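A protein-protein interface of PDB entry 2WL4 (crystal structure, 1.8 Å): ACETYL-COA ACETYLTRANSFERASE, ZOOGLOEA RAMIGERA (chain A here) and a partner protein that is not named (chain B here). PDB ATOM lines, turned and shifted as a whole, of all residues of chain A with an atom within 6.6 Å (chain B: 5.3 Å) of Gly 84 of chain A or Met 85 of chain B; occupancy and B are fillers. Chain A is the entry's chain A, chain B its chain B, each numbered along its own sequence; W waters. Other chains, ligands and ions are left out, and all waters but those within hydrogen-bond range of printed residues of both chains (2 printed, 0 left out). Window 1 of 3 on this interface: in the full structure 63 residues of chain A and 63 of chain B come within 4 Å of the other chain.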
ATOM      1  N   VAL A  52     -18.903   4.492  16.239  1.00  0.00           N
ATOM      2  CA  VAL A  52     -19.674   3.456  16.950  1.00  0.00           C
ATOM      3  C   VAL A  52     -19.261   3.479  18.419  1.00  0.00           C
ATOM      4  O   VAL A  52     -18.081   3.512  18.721  1.00  0.00           O
ATOM      5  CB  VAL A  52     -19.421   2.046  16.346  1.00  0.00           C
ATOM      6  CG1 VAL A  52     -20.068   0.942  17.196  1.00  0.00           C
ATOM      7  CG2 VAL A  52     -19.921   2.004  14.928  1.00  0.00           C
ATOM      8  N   ILE A  53     -20.236   3.534  19.324  1.00  0.00           N
ATOM      9  CA  ILE A  53     -19.965   3.578  20.782  1.00  0.00           C
ATOM     10  C   ILE A  53     -20.759   2.462  21.434  1.00  0.00           C
ATOM     11  O   ILE A  53     -21.987   2.495  21.415  1.00  0.00           O
ATOM     12  CB  ILE A  53     -20.445   4.922  21.398  1.00  0.00           C
ATOM     13  CG1 ILE A  53     -19.853   6.107  20.626  1.00  0.00           C
ATOM     14  CG2 ILE A  53     -20.135   4.997  22.907  1.00  0.00           C
ATOM     15  CD1 ILE A  53     -20.517   7.448  20.998  1.00  0.00           C
ATOM     16  N   LEU A  54     -20.065   1.479  22.013  1.00  0.00           N
ATOM     17  CA  LEU A  54     -20.714   0.299  22.584  1.00  0.00           C
ATOM     18  C   LEU A  54     -20.332   0.005  24.034  1.00  0.00           C
ATOM     19  O   LEU A  54     -19.179  -0.325  24.322  1.00  0.00           O
ATOM     20  CB  LEU A  54     -20.394  -0.946  21.748  1.00  0.00           C
ATOM     21  CG  LEU A  54     -21.040  -0.996  20.363  1.00  0.00           C
ATOM     22  CD1 LEU A  54     -20.340  -2.054  19.471  1.00  0.00           C
ATOM     23  CD2 LEU A  54     -22.576  -1.199  20.429  1.00  0.00           C
ATOM     24  N   GLY A  55     -21.325   0.072  24.927  1.00  0.00           N
ATOM     25  CA  GLY A  55     -21.133  -0.321  26.310  1.00  0.00           C
ATOM     26  C   GLY A  55     -20.795  -1.797  26.354  1.00  0.00           C
ATOM     27  O   GLY A  55     -21.362  -2.616  25.607  1.00  0.00           O
ATOM     28  N   GLN A  56     -19.864  -2.154  27.225  1.00  0.00           N
ATOM     29  CA  GLN A  56     -19.504  -3.556  27.370  1.00  0.00           C
ATOM     30  C   GLN A  56     -18.710  -3.669  28.652  1.00  0.00           C
ATOM     31  O   GLN A  56     -17.712  -2.956  28.872  1.00  0.00           O
ATOM     32  CB  GLN A  56     -18.701  -4.031  26.153  1.00  0.00           C
ATOM     33  CG  GLN A  56     -18.275  -5.500  26.276  1.00  0.00           C
ATOM     34  CD  GLN A  56     -17.481  -5.993  25.084  1.00  0.00           C
ATOM     35  OE1 GLN A  56     -17.058  -5.211  24.242  1.00  0.00           O
ATOM     36  NE2 GLN A  56     -17.261  -7.308  25.020  1.00  0.00           N
ATOM     37  N   ASN A  65     -10.177  -3.489  21.858  1.00  0.00           N
ATOM     38  CA  ASN A  65     -11.347  -2.636  21.570  1.00  0.00           C
ATOM     39  C   ASN A  65     -12.432  -3.317  20.724  1.00  0.00           C
ATOM     40  O   ASN A  65     -12.612  -2.983  19.554  1.00  0.00           O
ATOM     41  CB  ASN A  65     -10.865  -1.342  20.893  1.00  0.00           C
ATOM     42  CG  ASN A  65     -11.972  -0.313  20.695  1.00  0.00           C
ATOM     43  OD1 ASN A  65     -13.046  -0.378  21.310  1.00  0.00           O
ATOM     44  ND2 ASN A  65     -11.694   0.664  19.847  1.00  0.00           N
ATOM     45  N   PRO A  66     -13.181  -4.241  21.342  1.00  0.00           N
ATOM     46  CA  PRO A  66     -14.243  -4.980  20.650  1.00  0.00           C
ATOM     47  C   PRO A  66     -15.228  -4.081  19.884  1.00  0.00           C
ATOM     48  O   PRO A  66     -15.778  -4.535  18.889  1.00  0.00           O
ATOM     49  CB  PRO A  66     -14.922  -5.759  21.788  1.00  0.00           C
ATOM     50  CG  PRO A  66     -13.783  -6.025  22.734  1.00  0.00           C
ATOM     51  CD  PRO A  66     -12.915  -4.773  22.689  1.00  0.00           C
ATOM     52  N   ALA A  67     -15.459  -2.851  20.334  1.00  0.00           N
ATOM     53  CA  ALA A  67     -16.367  -1.929  19.612  1.00  0.00           C
ATOM     54  C   ALA A  67     -15.880  -1.733  18.187  1.00  0.00           C
ATOM     55  O   ALA A  67     -16.686  -1.658  17.243  1.00  0.00           O
ATOM     56  CB  ALA A  67     -16.438  -0.599  20.289  1.00  0.00           C
ATOM     57  N   ARG A  68     -14.559  -1.577  18.058  1.00  0.00           N
ATOM     58  CA  ARG A  68     -13.940  -1.386  16.740  1.00  0.00           C
ATOM     59  C   ARG A  68     -14.065  -2.673  15.901  1.00  0.00           C
ATOM     60  O   ARG A  68     -14.264  -2.622  14.687  1.00  0.00           O
ATOM     61  CB  ARG A  68     -12.478  -0.975  16.891  1.00  0.00           C
ATOM     62  CG  ARG A  68     -11.667  -0.888  15.570  1.00  0.00           C
ATOM     63  CD  ARG A  68     -12.120   0.260  14.634  1.00  0.00           C
ATOM     64  NE  ARG A  68     -11.043   0.637  13.687  1.00  0.00           N
ATOM     65  CZ  ARG A  68     -11.117   1.658  12.835  1.00  0.00           C
ATOM     66  NH1 ARG A  68     -12.222   2.351  12.757  1.00  0.00           N
ATOM     67  NH2 ARG A  68     -10.088   1.982  12.053  1.00  0.00           N
ATOM     68  N   ALA A  82     -14.314   4.090  16.822  1.00  0.00           N
ATOM     69  CA  ALA A  82     -15.187   3.313  17.707  1.00  0.00           C
ATOM     70  C   ALA A  82     -14.530   3.194  19.067  1.00  0.00           C
ATOM     71  O   ALA A  82     -13.315   3.202  19.162  1.00  0.00           O
ATOM     72  CB  ALA A  82     -15.419   1.913  17.142  1.00  0.00           C
ATOM     73  N   TRP A  83     -15.337   3.062  20.111  1.00  0.00           N
ATOM     74  CA  TRP A  83     -14.793   2.924  21.456  1.00  0.00           C
ATOM     75  C   TRP A  83     -15.796   2.228  22.369  1.00  0.00           C
ATOM     76  O   TRP A  83     -16.983   2.212  22.076  1.00  0.00           O
ATOM     77  CB  TRP A  83     -14.356   4.291  22.034  1.00  0.00           C
ATOM     78  CG  TRP A  83     -15.365   5.421  21.947  1.00  0.00           C
ATOM     79  CD1 TRP A  83     -15.635   6.191  20.868  1.00  0.00           C
ATOM     80  CD2 TRP A  83     -16.153   5.940  23.023  1.00  0.00           C
ATOM     81  NE1 TRP A  83     -16.564   7.146  21.186  1.00  0.00           N
ATOM     82  CE2 TRP A  83     -16.898   7.013  22.500  1.00  0.00           C
ATOM     83  CE3 TRP A  83     -16.297   5.599  24.364  1.00  0.00           C
ATOM     84  CZ2 TRP A  83     -17.796   7.742  23.288  1.00  0.00           C
ATOM     85  CZ3 TRP A  83     -17.193   6.323  25.140  1.00  0.00           C
ATOM     86  CH2 TRP A  83     -17.917   7.392  24.597  1.00  0.00           C
ATOM     87  N   GLY A  84     -15.304   1.575  23.423  1.00  0.00           N
ATOM     88  CA  GLY A  84     -16.191   0.937  24.377  1.00  0.00           C
ATOM     89  C   GLY A  84     -16.282   1.779  25.634  1.00  0.00           C
ATOM     90  O   GLY A  84     -15.438   2.648  25.887  1.00  0.00           O
ATOM     91  N   MET A  85     -17.359   1.607  26.389  1.00  0.00           N
ATOM     92  CA  MET A  85     -17.446   2.294  27.677  1.00  0.00           C
ATOM     93  C   MET A  85     -18.100   1.359  28.705  1.00  0.00           C
ATOM     94  O   MET A  85     -18.674   0.325  28.333  1.00  0.00           O
ATOM     95  CB  MET A  85     -18.097   3.717  27.568  1.00  0.00           C
ATOM     96  CG  MET A  85     -19.477   3.797  26.853  1.00  0.00           C
ATOM     97  SD  MET A  85     -20.861   3.228  27.861  1.00  0.00           S
ATOM     98  CE  MET A  85     -20.699   4.283  29.294  1.00  0.00           C
ATOM     99  N   ASN A  86     -17.978   1.696  29.985  1.00  0.00           N
ATOM    100  CA  ASN A  86     -18.504   0.868  31.069  1.00  0.00           C
ATOM    101  C   ASN A  86     -19.091   1.721  32.182  1.00  0.00           C
ATOM    102  O   ASN A  86     -18.352   2.352  32.946  1.00  0.00           O
ATOM    103  CB  ASN A  86     -17.371  -0.022  31.622  1.00  0.00           C
ATOM    104  CG  ASN A  86     -17.791  -0.873  32.791  1.00  0.00           C
ATOM    105  OD1 ASN A  86     -18.974  -1.058  33.056  1.00  0.00           O
ATOM    106  ND2 ASN A  86     -16.786  -1.430  33.508  1.00  0.00           N
ATOM    107  N   ILE B  53     -14.610  10.439  34.846  1.00  0.00           N
ATOM    108  CA  ILE B  53     -14.545   9.672  33.601  1.00  0.00           C
ATOM    109  C   ILE B  53     -13.091   9.214  33.399  1.00  0.00           C
ATOM    110  O   ILE B  53     -12.206  10.057  33.223  1.00  0.00           O
ATOM    111  CB  ILE B  53     -14.960  10.530  32.383  1.00  0.00           C
ATOM    112  CG1 ILE B  53     -16.315  11.225  32.623  1.00  0.00           C
ATOM    113  CG2 ILE B  53     -14.965   9.696  31.084  1.00  0.00           C
ATOM    114  CD1 ILE B  53     -16.710  12.212  31.479  1.00  0.00           C
ATOM    115  N   LEU B  54     -12.831   7.903  33.457  1.00  0.00           N
ATOM    116  CA  LEU B  54     -11.447   7.408  33.408  1.00  0.00           C
ATOM    117  C   LEU B  54     -11.198   6.343  32.341  1.00  0.00           C
ATOM    118  O   LEU B  54     -11.767   5.253  32.407  1.00  0.00           O
ATOM    119  CB  LEU B  54     -11.002   6.862  34.780  1.00  0.00           C
ATOM    120  CG  LEU B  54     -10.824   7.935  35.868  1.00  0.00           C
ATOM    121  CD1 LEU B  54     -10.594   7.226  37.213  1.00  0.00           C
ATOM    122  CD2 LEU B  54      -9.673   8.947  35.566  1.00  0.00           C
ATOM    123  N   GLY B  55     -10.326   6.667  31.380  1.00  0.00           N
ATOM    124  CA  GLY B  55      -9.878   5.715  30.391  1.00  0.00           C
ATOM    125  C   GLY B  55      -9.123   4.601  31.098  1.00  0.00           C
ATOM    126  O   GLY B  55      -8.355   4.862  32.024  1.00  0.00           O
ATOM    127  N   GLN B  56      -9.338   3.363  30.658  1.00  0.00           N
ATOM    128  CA  GLN B  56      -8.641   2.217  31.226  1.00  0.00           C
ATOM    129  C   GLN B  56      -8.863   1.031  30.309  1.00  0.00           C
ATOM    130  O   GLN B  56     -10.012   0.590  30.082  1.00  0.00           O
ATOM    131  CB  GLN B  56      -9.161   1.888  32.627  1.00  0.00           C
ATOM    132  CG  GLN B  56      -8.372   0.750  33.274  1.00  0.00           C
ATOM    133  CD  GLN B  56      -8.875   0.453  34.668  1.00  0.00           C
ATOM    134  OE1 GLN B  56      -9.931   0.931  35.054  1.00  0.00           O
ATOM    135  NE2 GLN B  56      -8.126  -0.354  35.422  1.00  0.00           N
ATOM    136  N   VAL B  57      -7.764   0.499  29.795  1.00  0.00           N
ATOM    137  CA  VAL B  57      -7.847  -0.551  28.792  1.00  0.00           C
ATOM    138  C   VAL B  57      -7.884  -1.937  29.427  1.00  0.00           C
ATOM    139  O   VAL B  57      -8.493  -2.858  28.899  1.00  0.00           O
ATOM    140  CB  VAL B  57      -6.668  -0.447  27.810  1.00  0.00           C
ATOM    141  CG1 VAL B  57      -6.770  -1.569  26.792  1.00  0.00           C
ATOM    142  CG2 VAL B  57      -6.656   0.957  27.129  1.00  0.00           C
ATOM    143  N   TRP B  83     -17.634   6.499  35.331  1.00  0.00           N
ATOM    144  CA  TRP B  83     -17.586   5.393  34.390  1.00  0.00           C
ATOM    145  C   TRP B  83     -16.236   5.294  33.737  1.00  0.00           C
ATOM    146  O   TRP B  83     -15.413   6.182  33.879  1.00  0.00           O
ATOM    147  CB  TRP B  83     -18.670   5.529  33.318  1.00  0.00           C
ATOM    148  CG  TRP B  83     -18.764   6.908  32.712  1.00  0.00           C
ATOM    149  CD1 TRP B  83     -19.259   8.024  33.314  1.00  0.00           C
ATOM    150  CD2 TRP B  83     -18.380   7.301  31.386  1.00  0.00           C
ATOM    151  NE1 TRP B  83     -19.221   9.077  32.452  1.00  0.00           N
ATOM    152  CE2 TRP B  83     -18.675   8.670  31.262  1.00  0.00           C
ATOM    153  CE3 TRP B  83     -17.833   6.632  30.292  1.00  0.00           C
ATOM    154  CZ2 TRP B  83     -18.426   9.392  30.089  1.00  0.00           C
ATOM    155  CZ3 TRP B  83     -17.586   7.351  29.115  1.00  0.00           C
ATOM    156  CH2 TRP B  83     -17.899   8.710  29.023  1.00  0.00           C
ATOM    157  N   GLY B  84     -16.003   4.170  33.074  1.00  0.00           N
ATOM    158  CA  GLY B  84     -14.716   3.903  32.447  1.00  0.00           C
ATOM    159  C   GLY B  84     -14.933   3.890  30.946  1.00  0.00           C
ATOM    160  O   GLY B  84     -16.044   3.661  30.471  1.00  0.00           O
ATOM    161  N   MET B  85     -13.896   4.198  30.192  1.00  0.00           N
ATOM    162  CA  MET B  85     -14.006   4.096  28.744  1.00  0.00           C
ATOM    163  C   MET B  85     -12.716   3.586  28.130  1.00  0.00           C
ATOM    164  O   MET B  85     -11.674   3.563  28.785  1.00  0.00           O
ATOM    165  CB  MET B  85     -14.555   5.375  28.065  1.00  0.00           C
ATOM    166  CG  MET B  85     -13.826   6.688  28.394  1.00  0.00           C
ATOM    167  SD  MET B  85     -12.269   6.790  27.499  1.00  0.00           S
ATOM    168  CE  MET B  85     -12.827   6.676  25.777  1.00  0.00           C
ATOM    169  N   ASN B  86     -12.807   3.110  26.894  1.00  0.00           N
ATOM    170  CA  ASN B  86     -11.671   2.482  26.229  1.00  0.00           C
ATOM    171  C   ASN B  86     -11.656   2.855  24.743  1.00  0.00           C
ATOM    172  O   ASN B  86     -12.441   2.334  23.954  1.00  0.00           O
ATOM    173  CB  ASN B  86     -11.717   0.944  26.423  1.00  0.00           C
ATOM    174  CG  ASN B  86     -10.612   0.208  25.673  1.00  0.00           C
ATOM    175  OD1 ASN B  86      -9.600   0.791  25.306  1.00  0.00           O
ATOM    176  ND2 ASN B  86     -10.802  -1.105  25.463  1.00  0.00           N
ATOM    177  N   GLN B  87     -10.752   3.766  24.387  1.00  0.00           N
ATOM    178  CA  GLN B  87     -10.336   3.944  23.004  1.00  0.00           C
ATOM    179  C   GLN B  87      -8.826   3.699  22.942  1.00  0.00           C
ATOM    180  O   GLN B  87      -8.075   4.479  22.370  1.00  0.00           O
ATOM    181  CB  GLN B  87     -10.732   5.310  22.444  1.00  0.00           C
ATOM    182  CG  GLN B  87     -10.770   5.347  20.931  1.00  0.00           C
ATOM    183  CD  GLN B  87     -11.238   6.708  20.414  1.00  0.00           C
ATOM    184  OE1 GLN B  87     -11.523   7.629  21.199  1.00  0.00           O
ATOM    185  NE2 GLN B  87     -11.262   6.853  19.100  1.00  0.00           N
ATOM    186  N   SER B  91      -7.311   6.741  25.089  1.00  0.00           N
ATOM    187  CA  SER B  91      -8.346   6.818  26.105  1.00  0.00           C
ATOM    188  C   SER B  91      -8.286   8.026  27.051  1.00  0.00           C
ATOM    189  O   SER B  91      -9.318   8.673  27.291  1.00  0.00           O
ATOM    190  CB  SER B  91      -8.370   5.531  26.924  1.00  0.00           C
ATOM    191  OG  SER B  91      -8.819   4.441  26.132  1.00  0.00           O
ATOM    192  N   ARG B  94      -9.194  11.123  25.087  1.00  0.00           N
ATOM    193  CA  ARG B  94     -10.608  11.068  24.732  1.00  0.00           C
ATOM    194  C   ARG B  94     -11.500  11.336  25.936  1.00  0.00           C
ATOM    195  O   ARG B  94     -12.502  12.036  25.818  1.00  0.00           O
ATOM    196  CB  ARG B  94     -10.968   9.721  24.087  1.00  0.00           C
ATOM    197  CG  ARG B  94     -12.413   9.633  23.671  1.00  0.00           C
ATOM    198  CD  ARG B  94     -12.615  10.582  22.507  1.00  0.00           C
ATOM    199  NE  ARG B  94     -14.008  10.826  22.130  1.00  0.00           N
ATOM    200  CZ  ARG B  94     -14.638  10.130  21.193  1.00  0.00           C
ATOM    201  NH1 ARG B  94     -14.003   9.122  20.593  1.00  0.00           N
ATOM    202  NH2 ARG B  94     -15.891  10.429  20.862  1.00  0.00           N
ATOM    203  N   ALA B  95     -11.133  10.804  27.098  1.00  0.00           N
ATOM    204  CA  ALA B  95     -11.900  11.040  28.315  1.00  0.00           C
ATOM    205  C   ALA B  95     -12.059  12.513  28.656  1.00  0.00           C
ATOM    206  O   ALA B  95     -13.110  12.918  29.150  1.00  0.00           O
ATOM    207  CB  ALA B  95     -11.279  10.266  29.519  1.00  0.00           C
ATOM    208  N   LEU B  98     -14.564  13.885  26.237  1.00  0.00           N
ATOM    209  CA  LEU B  98     -15.878  13.426  26.670  1.00  0.00           C
ATOM    210  C   LEU B  98     -16.362  14.201  27.909  1.00  0.00           C
ATOM    211  O   LEU B  98     -17.533  14.538  28.010  1.00  0.00           O
ATOM    212  CB  LEU B  98     -15.861  11.904  26.926  1.00  0.00           C
ATOM    213  CG  LEU B  98     -15.789  10.999  25.677  1.00  0.00           C
ATOM    214  CD1 LEU B  98     -15.263   9.581  26.108  1.00  0.00           C
ATOM    215  CD2 LEU B  98     -17.170  10.868  24.999  1.00  0.00           C
HETATM  216  O   HOH W   1      -9.149  -3.284  24.525  1.00  0.00           O
HETATM  217  O   HOH W   2     -14.834   0.911  28.833  1.00  0.00           O
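O of Gly 84 of chain A sits at hydrogen-bond distance from N of Asn 86 of chain B, 2.9 Å away. N of Asn 86 of chain A sits at hydrogen-bond distance from O of Gly 84 of chain B. NE1 of Trp 83 of chain A lies close to NH1 of Arg 94 of chain B (3.3 Å).
The backbone carbonyl oxygen (O) of Trp 83 of chain A lies within hydrogen-bond range of the backbone NH (N) of Leu 54 of chain A (3.2 Å). O of Leu 54 of chain A is in hydrogen-bond range of N of Met 85 of chain A (3.4 Å). The backbone NH (N) of Leu 54 of chain B lies within hydrogen-bond range of the backbone carbonyl oxygen (O) of Trp 83 of chain B. The backbone NH of Gln 56 of chain B is in hydrogen-bond range of the backbone carbonyl oxygen of Met 85 of chain B (3.0 Å). The backbone NH (N) of Gln 87 of chain B is in hydrogen-bond range of the side-chain hydroxyl (OG) of Ser 91 of chain B (2.7 Å). NH1 of Arg 94 of chain B is in hydrogen-bond range of OE1 of Gln 87 of chain B, at 3.0 Å.
Asn 65 of chain A touches Asn 86 of chain B (OD1 to O, 3.8 Å). Ala 82 of chain A touches Gln 87 of chain B (O to CG, 3.8 Å). Met 85 of chain B touches Trp 83 of chain A. Trp 83 of chain A touches Asn 86 of chain B. Gln 87 of chain B touches Trp 83 of chain A. Leu 98 of chain B touches Trp 83 of chain A. Met 85 of chain B touches Gly 84 of chain A. Met 85 of chain A touches Trp 83 of chain B (CE to CE3, 3.8 Å). CA of Met 85 of chain A touches O of Gly 84 of chain B (3.4 Å). Met 85 of chain A touches Met 85 of chain B.
Of the printed residues of chain A, Gln 87 of chain B touches Ala 82 (3.8 Å) and Trp 83 (3.8 Å). Of the printed residues of chain B, Ala 82 of chain A touches Gln 87. Of the printed residues of chain B, Trp 83 of chain A touches Met 85, Asn 86, Gln 87, Arg 94 and Leu 98. Of the printed residues of chain B, Asn 86 of chain A touches Trp 83 (3.2 Å) and Gly 84 (2.8 Å). Of the printed residues of chain B, Asn 65 of chain A touches Asn 86 (3.8 Å). Val 52 of chain A touches none of the printed residues of chain B. The nearest residue of chain B that does not touch Gly 84 of chain A is Gly 84 of chain B (4.7 Å).
Hydrophobic or aromatic side chains of chain B within 4 Å of the printed part of chain A: Trp 83, Met 85 and Leu 98. Along chain B the printed residues that touch a printed residue of chain A span positions 83 to 98. Of the 14 printed residues of chain A, 6 touch a printed residue of chain B. Among the printed residues, 14 pairs touch across the chains. Among the printed residues, no Asp or Glu carboxylate lies within 4 Å of a Lys or Arg side-chain nitrogen of the other chain.
Water W1 lies within hydrogen-bond range of N of Asn 65 of chain A (2.9 Å) and ND2 of Asn 86 of chain B (2.9 Å). Water W2 lies within hydrogen-bond range of the backbone carbonyl oxygen of Gly 84 of chain B, the backbone NH of Asn 86 of chain A and the backbone carbonyl oxygen of Gly 84 of chain A.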
